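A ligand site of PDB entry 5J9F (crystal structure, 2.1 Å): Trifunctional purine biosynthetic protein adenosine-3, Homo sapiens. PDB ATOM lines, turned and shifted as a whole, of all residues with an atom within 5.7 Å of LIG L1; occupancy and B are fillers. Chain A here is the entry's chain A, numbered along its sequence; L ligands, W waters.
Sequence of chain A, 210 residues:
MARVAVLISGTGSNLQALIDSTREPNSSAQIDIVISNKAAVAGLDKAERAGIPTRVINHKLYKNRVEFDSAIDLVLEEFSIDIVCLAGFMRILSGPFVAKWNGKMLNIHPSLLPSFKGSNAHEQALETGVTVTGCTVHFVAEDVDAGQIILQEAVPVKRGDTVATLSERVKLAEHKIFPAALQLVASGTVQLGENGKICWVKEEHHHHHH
A nitrogen (N5) of LIG L1 sits close to a nitrogen (N2) of LG2 L2, at 3.2 Å.
NH1 of Arg 65 is in salt-bridge range of O4 of LIG L1, at 3.9 Å. An oxygen (O4) of LIG L1 is in salt-bridge range of the guanidinium group of Arg 91. The backbone carbonyl oxygen (O) of Leu 93 lies within hydrogen-bond range of a nitrogen (N3) of LIG L1, 3.1 Å away. O1 of LIG L1 sits at hydrogen-bond distance from N of Asp 145 (2.9 Å). The backbone carbonyl oxygen (O) of Arg 91 sits at hydrogen-bond distance from a nitrogen (N4) of LIG L1, at 2.9 Å. A nitrogen (N3) of LIG L1 sits at hydrogen-bond distance from the backbone carbonyl oxygen (O) of Glu 142 (3.1 Å). The backbone NH (N) of Leu 93 lies within hydrogen-bond range of a nitrogen (N2) of LIG L1, at 3.1 Å. The backbone carbonyl oxygen (O) of Ala 141 is in hydrogen-bond range of a nitrogen (N1) of LIG L1 (2.8 Å). An oxygen (O4) of LIG L1 lies within hydrogen-bond range of the backbone NH (N) of Ile 92 (3.2 Å).
Water W2 lies within hydrogen-bond range of OD1 of Asp 145, ND1 of His 109, N2 of LG2 L2, N5 of LIG L1 and ND2 of Asn 107.
The backbone NH of Ile 108 sits at hydrogen-bond distance from the backbone carbonyl oxygen of Leu 86 (3.4 Å). The backbone NH (N) of Asn 107 is in hydrogen-bond range of the backbone carbonyl oxygen (O) of His 138 (2.9 Å). A ring nitrogen (ND1) of His 109 lies close to the side-chain carboxylate of Asp 145 (3.4 Å). The backbone NH (N) of Gly 118 sits at hydrogen-bond distance from the side-chain carboxylate (OD2) of Asp 145, at 2.8 Å.
Residues that only touch LIG L1: Phe 89 (3.2 Å), Met 90 (3.4 Å), Val 140 (3.5 Å), Asn 107 (3.6 Å), His 138 (3.6 Å), Val 144 (3.7 Å), Val 98 (3.7 Å), Ser 119 (3.9 Å), Asp 143 (3.97 Å) and Leu 86 (3.97 Å). Hydrophobic or aromatic side chains that line LIG L1: Leu 86, Ile 92, Leu 93, Val 98, His 138, Val 140 and Val 144.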
ATOM      1  N   ARG A  65       1.153  12.396  -1.809  1.00  0.00           N
ATOM      2  CA  ARG A  65       1.450  12.579  -0.396  1.00  0.00           C
ATOM      3  C   ARG A  65       2.821  11.992   0.005  1.00  0.00           C
ATOM      4  O   ARG A  65       3.610  12.646   0.683  1.00  0.00           O
ATOM      5  CB  ARG A  65       0.343  11.964   0.448  1.00  0.00           C
ATOM      6  CG  ARG A  65       0.112  12.634   1.767  1.00  0.00           C
ATOM      7  CD  ARG A  65      -1.283  13.230   1.807  1.00  0.00           C
ATOM      8  NE  ARG A  65      -2.320  12.235   1.552  1.00  0.00           N
ATOM      9  CZ  ARG A  65      -3.616  12.520   1.464  1.00  0.00           C
ATOM     10  NH1 ARG A  65      -4.033  13.769   1.595  1.00  0.00           N
ATOM     11  NH2 ARG A  65      -4.471  11.540   1.223  1.00  0.00           N
ATOM     12  N   LEU A  86       2.561  19.192  15.156  1.00  0.00           N
ATOM     13  CA  LEU A  86       1.728  19.766  14.090  1.00  0.00           C
ATOM     14  C   LEU A  86       0.894  20.899  14.682  1.00  0.00           C
ATOM     15  O   LEU A  86       0.063  20.652  15.535  1.00  0.00           O
ATOM     16  CB  LEU A  86       0.832  18.697  13.477  1.00  0.00           C
ATOM     17  CG  LEU A  86       1.552  17.417  13.043  1.00  0.00           C
ATOM     18  CD1 LEU A  86       0.629  16.500  12.302  1.00  0.00           C
ATOM     19  CD2 LEU A  86       2.764  17.745  12.171  1.00  0.00           C
ATOM     20  N   PHE A  89      -1.052  22.771  11.204  1.00  0.00           N
ATOM     21  CA  PHE A  89      -0.626  22.128   9.960  1.00  0.00           C
ATOM     22  C   PHE A  89      -1.845  21.450   9.338  1.00  0.00           C
ATOM     23  O   PHE A  89      -2.463  20.600   9.976  1.00  0.00           O
ATOM     24  CB  PHE A  89       0.476  21.103  10.227  1.00  0.00           C
ATOM     25  CG  PHE A  89       1.094  20.509   8.988  1.00  0.00           C
ATOM     26  CD1 PHE A  89       1.888  21.288   8.146  1.00  0.00           C
ATOM     27  CD2 PHE A  89       0.876  19.176   8.666  1.00  0.00           C
ATOM     28  CE1 PHE A  89       2.468  20.721   7.009  1.00  0.00           C
ATOM     29  CE2 PHE A  89       1.440  18.611   7.536  1.00  0.00           C
ATOM     30  CZ  PHE A  89       2.245  19.383   6.720  1.00  0.00           C
ATOM     31  N   MET A  90      -2.214  21.824   8.125  1.00  0.00           N
ATOM     32  CA  MET A  90      -3.496  21.329   7.603  1.00  0.00           C
ATOM     33  C   MET A  90      -3.399  20.242   6.527  1.00  0.00           C
ATOM     34  O   MET A  90      -4.263  20.167   5.636  1.00  0.00           O
ATOM     35  CB  MET A  90      -4.323  22.502   7.055  1.00  0.00           C
ATOM     36  CG  MET A  90      -4.678  23.572   8.085  1.00  0.00           C
ATOM     37  SD  MET A  90      -5.471  22.917   9.609  1.00  0.00           S
ATOM     38  CE  MET A  90      -7.098  22.430   8.998  1.00  0.00           C
ATOM     39  N   ARG A  91      -2.381  19.376   6.611  1.00  0.00           N
ATOM     40  CA  ARG A  91      -2.293  18.259   5.650  1.00  0.00           C
ATOM     41  C   ARG A  91      -2.440  16.921   6.373  1.00  0.00           C
ATOM     42  O   ARG A  91      -1.962  16.752   7.495  1.00  0.00           O
ATOM     43  CB  ARG A  91      -0.974  18.275   4.876  1.00  0.00           C
ATOM     44  CG  ARG A  91      -0.704  19.538   4.112  1.00  0.00           C
ATOM     45  CD  ARG A  91      -1.800  19.797   3.086  1.00  0.00           C
ATOM     46  NE  ARG A  91      -1.849  18.741   2.072  1.00  0.00           N
ATOM     47  CZ  ARG A  91      -2.728  18.709   1.080  1.00  0.00           C
ATOM     48  NH1 ARG A  91      -3.632  19.685   0.978  1.00  0.00           N
ATOM     49  NH2 ARG A  91      -2.703  17.712   0.187  1.00  0.00           N
ATOM     50  N   ILE A  92      -3.058  15.961   5.706  1.00  0.00           N
ATOM     51  CA  ILE A  92      -3.091  14.598   6.200  1.00  0.00           C
ATOM     52  C   ILE A  92      -1.770  13.940   5.849  1.00  0.00           C
ATOM     53  O   ILE A  92      -1.317  14.072   4.729  1.00  0.00           O
ATOM     54  CB  ILE A  92      -4.293  13.850   5.614  1.00  0.00           C
ATOM     55  CG1 ILE A  92      -5.570  14.365   6.263  1.00  0.00           C
ATOM     56  CG2 ILE A  92      -4.155  12.348   5.809  1.00  0.00           C
ATOM     57  CD1 ILE A  92      -6.858  13.845   5.643  1.00  0.00           C
ATOM     58  N   LEU A  93      -1.117  13.274   6.800  1.00  0.00           N
ATOM     59  CA  LEU A  93       0.183  12.640   6.545  1.00  0.00           C
ATOM     60  C   LEU A  93       0.041  11.168   6.121  1.00  0.00           C
ATOM     61  O   LEU A  93      -0.855  10.474   6.577  1.00  0.00           O
ATOM     62  CB  LEU A  93       1.063  12.743   7.801  1.00  0.00           C
ATOM     63  CG  LEU A  93       1.443  14.169   8.214  1.00  0.00           C
ATOM     64  CD1 LEU A  93       1.976  14.176   9.606  1.00  0.00           C
ATOM     65  CD2 LEU A  93       2.522  14.698   7.287  1.00  0.00           C
ATOM     66  N   SER A  94       0.940  10.693   5.270  1.00  0.00           N
ATOM     67  CA  SER A  94       0.883   9.298   4.792  1.00  0.00           C
ATOM     68  C   SER A  94       1.232   8.286   5.871  1.00  0.00           C
ATOM     69  O   SER A  94       1.996   8.563   6.828  1.00  0.00           O
ATOM     70  CB  SER A  94       1.832   9.095   3.616  1.00  0.00           C
ATOM     71  OG  SER A  94       3.199   9.279   4.008  1.00  0.00           O
ATOM     72  N   VAL A  98       3.847   8.459   9.170  1.00  0.00           N
ATOM     73  CA  VAL A  98       3.264   8.322  10.494  1.00  0.00           C
ATOM     74  C   VAL A  98       3.868   7.144  11.285  1.00  0.00           C
ATOM     75  O   VAL A  98       4.097   7.263  12.496  1.00  0.00           O
ATOM     76  CB  VAL A  98       1.729   8.173  10.404  1.00  0.00           C
ATOM     77  CG1 VAL A  98       1.108   7.983  11.794  1.00  0.00           C
ATOM     78  CG2 VAL A  98       1.132   9.395   9.749  1.00  0.00           C
ATOM     79  N   ASN A 107      -0.164  16.400  17.700  1.00  0.00           N
ATOM     80  CA  ASN A 107      -1.060  17.292  16.945  1.00  0.00           C
ATOM     81  C   ASN A 107      -1.957  18.061  17.923  1.00  0.00           C
ATOM     82  O   ASN A 107      -2.329  17.499  18.963  1.00  0.00           O
ATOM     83  CB  ASN A 107      -1.921  16.503  15.959  1.00  0.00           C
ATOM     84  CG  ASN A 107      -2.909  17.389  15.203  1.00  0.00           C
ATOM     85  OD1 ASN A 107      -2.498  18.314  14.508  1.00  0.00           O
ATOM     86  ND2 ASN A 107      -4.209  17.056  15.296  1.00  0.00           N
ATOM     87  N   ILE A 108      -2.295  19.305  17.632  1.00  0.00           N
ATOM     88  CA  ILE A 108      -3.335  20.018  18.424  1.00  0.00           C
ATOM     89  C   ILE A 108      -4.630  20.077  17.570  1.00  0.00           C
ATOM     90  O   ILE A 108      -4.585  20.399  16.365  1.00  0.00           O
ATOM     91  CB  ILE A 108      -2.853  21.432  18.879  1.00  0.00           C
ATOM     92  CG1 ILE A 108      -3.930  22.183  19.674  1.00  0.00           C
ATOM     93  CG2 ILE A 108      -2.464  22.312  17.674  1.00  0.00           C
ATOM     94  CD1 ILE A 108      -4.131  21.722  21.081  1.00  0.00           C
ATOM     95  N   HIS A 109      -5.763  19.723  18.165  1.00  0.00           N
ATOM     96  CA  HIS A 109      -7.048  19.676  17.443  1.00  0.00           C
ATOM     97  C   HIS A 109      -8.123  20.447  18.275  1.00  0.00           C
ATOM     98  O   HIS A 109      -8.272  20.218  19.486  1.00  0.00           O
ATOM     99  CB  HIS A 109      -7.490  18.228  17.208  1.00  0.00           C
ATOM    100  CG  HIS A 109      -8.808  18.113  16.482  1.00  0.00           C
ATOM    101  ND1 HIS A 109      -8.909  18.155  15.111  1.00  0.00           N
ATOM    102  CD2 HIS A 109     -10.072  18.006  16.953  1.00  0.00           C
ATOM    103  CE1 HIS A 109     -10.176  18.047  14.752  1.00  0.00           C
ATOM    104  NE2 HIS A 109     -10.907  17.983  15.859  1.00  0.00           N
ATOM    105  N   GLY A 118     -11.689  16.159  12.117  1.00  0.00           N
ATOM    106  CA  GLY A 118     -11.593  16.775  10.813  1.00  0.00           C
ATOM    107  C   GLY A 118     -11.266  18.255  10.859  1.00  0.00           C
ATOM    108  O   GLY A 118     -10.939  18.783  11.920  1.00  0.00           O
ATOM    109  N   SER A 119     -11.409  18.927   9.712  1.00  0.00           N
ATOM    110  CA  SER A 119     -10.747  20.208   9.515  1.00  0.00           C
ATOM    111  C   SER A 119     -11.607  21.427   9.841  1.00  0.00           C
ATOM    112  O   SER A 119     -11.087  22.550   9.811  1.00  0.00           O
ATOM    113  CB  SER A 119     -10.281  20.332   8.070  1.00  0.00           C
ATOM    114  OG  SER A 119     -11.413  20.355   7.232  1.00  0.00           O
ATOM    115  N   HIS A 138      -2.837  15.119  20.874  1.00  0.00           N
ATOM    116  CA  HIS A 138      -2.767  13.686  20.791  1.00  0.00           C
ATOM    117  C   HIS A 138      -1.572  13.255  19.963  1.00  0.00           C
ATOM    118  O   HIS A 138      -1.058  14.023  19.133  1.00  0.00           O
ATOM    119  CB  HIS A 138      -4.062  13.145  20.176  1.00  0.00           C
ATOM    120  CG  HIS A 138      -4.321  13.637  18.781  1.00  0.00           C
ATOM    121  ND1 HIS A 138      -3.940  12.930  17.658  1.00  0.00           N
ATOM    122  CD2 HIS A 138      -4.883  14.782  18.327  1.00  0.00           C
ATOM    123  CE1 HIS A 138      -4.295  13.615  16.579  1.00  0.00           C
ATOM    124  NE2 HIS A 138      -4.859  14.737  16.951  1.00  0.00           N
ATOM    125  N   PHE A 139      -1.122  12.035  20.221  1.00  0.00           N
ATOM    126  CA  PHE A 139      -0.162  11.389  19.330  1.00  0.00           C
ATOM    127  C   PHE A 139      -0.799  11.159  17.952  1.00  0.00           C
ATOM    128  O   PHE A 139      -1.975  10.851  17.833  1.00  0.00           O
ATOM    129  CB  PHE A 139       0.313  10.049  19.909  1.00  0.00           C
ATOM    130  CG  PHE A 139       1.356  10.201  20.984  1.00  0.00           C
ATOM    131  CD1 PHE A 139       2.624  10.645  20.658  1.00  0.00           C
ATOM    132  CD2 PHE A 139       1.071   9.899  22.303  1.00  0.00           C
ATOM    133  CE1 PHE A 139       3.594  10.787  21.649  1.00  0.00           C
ATOM    134  CE2 PHE A 139       2.015  10.021  23.276  1.00  0.00           C
ATOM    135  CZ  PHE A 139       3.299  10.462  22.943  1.00  0.00           C
ATOM    136  N   VAL A 140      -0.015  11.336  16.902  1.00  0.00           N
ATOM    137  CA  VAL A 140      -0.538  11.181  15.560  1.00  0.00           C
ATOM    138  C   VAL A 140      -0.460   9.702  15.152  1.00  0.00           C
ATOM    139  O   VAL A 140       0.620   9.106  15.158  1.00  0.00           O
ATOM    140  CB  VAL A 140       0.252  12.068  14.544  1.00  0.00           C
ATOM    141  CG1 VAL A 140      -0.243  11.843  13.124  1.00  0.00           C
ATOM    142  CG2 VAL A 140       0.069  13.516  14.893  1.00  0.00           C
ATOM    143  N   ALA A 141      -1.604   9.118  14.873  1.00  0.00           N
ATOM    144  CA  ALA A 141      -1.661   7.779  14.292  1.00  0.00           C
ATOM    145  C   ALA A 141      -2.138   7.906  12.833  1.00  0.00           C
ATOM    146  O   ALA A 141      -2.472   9.001  12.357  1.00  0.00           O
ATOM    147  CB  ALA A 141      -2.598   6.866  15.101  1.00  0.00           C
ATOM    148  N   GLU A 142      -2.190   6.789  12.137  1.00  0.00           N
ATOM    149  CA  GLU A 142      -2.523   6.822  10.742  1.00  0.00           C
ATOM    150  C   GLU A 142      -3.965   7.228  10.560  1.00  0.00           C
ATOM    151  O   GLU A 142      -4.275   8.079   9.721  1.00  0.00           O
ATOM    152  CB  GLU A 142      -2.240   5.467  10.092  1.00  0.00           C
ATOM    153  CG  GLU A 142      -2.199   5.570   8.575  1.00  0.00           C
ATOM    154  CD  GLU A 142      -1.726   4.288   7.889  1.00  0.00           C
ATOM    155  OE1 GLU A 142      -0.971   3.492   8.515  1.00  0.00           O
ATOM    156  OE2 GLU A 142      -2.131   4.083   6.721  1.00  0.00           O
ATOM    157  N   ASP A 143      -4.843   6.644  11.356  1.00  0.00           N
ATOM    158  CA  ASP A 143      -6.223   7.083  11.417  1.00  0.00           C
ATOM    159  C   ASP A 143      -6.348   8.545  11.951  1.00  0.00           C
ATOM    160  O   ASP A 143      -5.917   8.858  13.067  1.00  0.00           O
ATOM    161  CB  ASP A 143      -7.002   6.103  12.284  1.00  0.00           C
ATOM    162  CG  ASP A 143      -8.487   6.221  12.104  1.00  0.00           C
ATOM    163  OD1 ASP A 143      -8.918   6.790  11.072  1.00  0.00           O
ATOM    164  OD2 ASP A 143      -9.220   5.736  13.008  1.00  0.00           O
ATOM    165  N   VAL A 144      -6.928   9.420  11.146  1.00  0.00           N
ATOM    166  CA  VAL A 144      -6.867  10.861  11.397  1.00  0.00           C
ATOM    167  C   VAL A 144      -7.603  11.324  12.682  1.00  0.00           C
ATOM    168  O   VAL A 144      -8.738  10.945  12.922  1.00  0.00           O
ATOM    169  CB  VAL A 144      -7.423  11.600  10.172  1.00  0.00           C
ATOM    170  CG1 VAL A 144      -7.475  13.097  10.408  1.00  0.00           C
ATOM    171  CG2 VAL A 144      -6.570  11.256   8.942  1.00  0.00           C
ATOM    172  N   ASP A 145      -6.928  12.124  13.528  1.00  0.00           N
ATOM    173  CA  ASP A 145      -7.510  12.626  14.782  1.00  0.00           C
ATOM    174  C   ASP A 145      -7.994  11.488  15.663  1.00  0.00           C
ATOM    175  O   ASP A 145      -8.958  11.639  16.428  1.00  0.00           O
ATOM    176  CB  ASP A 145      -8.704  13.588  14.521  1.00  0.00           C
ATOM    177  CG  ASP A 145      -8.304  14.858  13.743  1.00  0.00           C
ATOM    178  OD1 ASP A 145      -7.095  15.263  13.772  1.00  0.00           O
ATOM    179  OD2 ASP A 145      -9.201  15.451  13.097  1.00  0.00           O
ATOM    180  N   ALA A 146      -7.330  10.338  15.581  1.00  0.00           N
ATOM    181  CA  ALA A 146      -7.721   9.191  16.373  1.00  0.00           C
ATOM    182  C   ALA A 146      -6.572   8.647  17.235  1.00  0.00           C
ATOM    183  O   ALA A 146      -6.781   7.694  17.972  1.00  0.00           O
ATOM    184  CB  ALA A 146      -8.290   8.051  15.453  1.00  0.00           C
ATOM    185  N   GLY A 147      -5.376   9.240  17.179  1.00  0.00           N
ATOM    186  CA  GLY A 147      -4.244   8.758  17.954  1.00  0.00           C
ATOM    187  C   GLY A 147      -4.469   8.917  19.462  1.00  0.00           C
ATOM    188  O   GLY A 147      -5.486   9.475  19.894  1.00  0.00           O
HETATM  189  C1  LIG L   1      -3.328  13.852  11.526  1.00  0.00           C
HETATM  190  N1  LIG L   1      -3.196  11.516  11.279  1.00  0.00           N
HETATM  191  O1  LIG L   1      -4.055  12.365  13.174  1.00  0.00           O
HETATM  192  C2  LIG L   1      -3.538  12.573  12.039  1.00  0.00           C
HETATM  193  N2  LIG L   1      -2.431  12.862   9.545  1.00  0.00           N
HETATM  194  O2  LIG L   1      -9.214  17.398   5.721  1.00  0.00           O
HETATM  195  C3  LIG L   1      -2.677  11.650  10.052  1.00  0.00           C
HETATM  196  N3  LIG L   1      -2.327  10.499   9.303  1.00  0.00           N
HETATM  197  O3  LIG L   1      -6.576  16.780   1.778  1.00  0.00           O
HETATM  198  C4  LIG L   1      -2.749  13.955  10.233  1.00  0.00           C
HETATM  199  N4  LIG L   1      -2.619  15.247   9.916  1.00  0.00           N
HETATM  200  O4  LIG L   1      -5.076  17.026   3.406  1.00  0.00           O
HETATM  201  C5  LIG L   1      -3.058  16.076  10.883  1.00  0.00           C
HETATM  202  N5  LIG L   1      -5.495  17.496  11.051  1.00  0.00           N
HETATM  203  O5  LIG L   1      -8.704  21.498   1.384  1.00  0.00           O
HETATM  204  C6  LIG L   1      -3.502  15.190  11.879  1.00  0.00           C
HETATM  205  N6  LIG L   1      -7.053  18.027   4.998  1.00  0.00           N
HETATM  206  O6  LIG L   1      -7.368  22.732   2.608  1.00  0.00           O
HETATM  207  C7  LIG L   1      -3.025  17.590  10.786  1.00  0.00           C
HETATM  208  C8  LIG L   1      -4.270  18.238  11.387  1.00  0.00           C
HETATM  209  C9  LIG L   1      -6.172  17.502   9.802  1.00  0.00           C
HETATM  210  C10 LIG L   1      -7.324  16.723   9.607  1.00  0.00           C
HETATM  211  C11 LIG L   1      -7.951  16.750   8.359  1.00  0.00           C
HETATM  212  C12 LIG L   1      -7.428  17.568   7.366  1.00  0.00           C
HETATM  213  C13 LIG L   1      -6.294  18.343   7.591  1.00  0.00           C
HETATM  214  C14 LIG L   1      -5.664  18.323   8.816  1.00  0.00           C
HETATM  215  C15 LIG L   1      -8.041  17.656   5.962  1.00  0.00           C
HETATM  216  C16 LIG L   1      -7.182  18.209   3.598  1.00  0.00           C
HETATM  217  C17 LIG L   1      -6.229  17.282   2.893  1.00  0.00           C
HETATM  218  C18 LIG L   1      -6.801  19.642   3.253  1.00  0.00           C
HETATM  219  C19 LIG L   1      -7.986  20.576   3.503  1.00  0.00           C
HETATM  220  C20 LIG L   1      -8.017  21.667   2.438  1.00  0.00           C
HETATM  221  C1  LG2 L   2      -5.618  26.015  15.724  1.00  0.00           C
HETATM  222  O1  LG2 L   2      -6.862  26.301  16.335  1.00  0.00           O
HETATM  223  C2  LG2 L   2      -5.553  24.508  15.599  1.00  0.00           C
HETATM  224  O2  LG2 L   2      -6.078  23.814  16.722  1.00  0.00           O
HETATM  225  C3  LG2 L   2      -6.364  24.230  14.337  1.00  0.00           C
HETATM  226  O3  LG2 L   2      -5.936  25.289  13.505  1.00  0.00           O
HETATM  227  C4  LG2 L   2      -5.638  26.467  14.273  1.00  0.00           C
HETATM  228  C5  LG2 L   2      -4.258  26.957  13.865  1.00  0.00           C
HETATM  229  O4  LG2 L   2      -3.991  28.194  14.536  1.00  0.00           O
HETATM  230  N1  LG2 L   2      -5.932  22.955  13.780  1.00  0.00           N
HETATM  231  C6  LG2 L   2      -6.803  22.139  13.195  1.00  0.00           C
HETATM  232  O5  LG2 L   2      -7.977  22.447  12.960  1.00  0.00           O
HETATM  233  C7  LG2 L   2      -6.241  20.773  12.828  1.00  0.00           C
HETATM  234  N2  LG2 L   2      -7.206  19.961  12.109  1.00  0.00           N
HETATM  235  P1  LG2 L   2      -2.484  28.822  14.634  1.00  0.00           P
HETATM  236  O6  LG2 L   2      -1.722  27.917  15.616  1.00  0.00           O
HETATM  237  O7  LG2 L   2      -2.737  30.216  15.180  1.00  0.00           O
HETATM  238  O8  LG2 L   2      -1.905  28.777  13.230  1.00  0.00           O
HETATM  239  O   HOH W   1      -4.382  10.306  14.732  1.00  0.00           O
HETATM  240  O   HOH W   2      -6.704  17.700  13.707  1.00  0.00           O
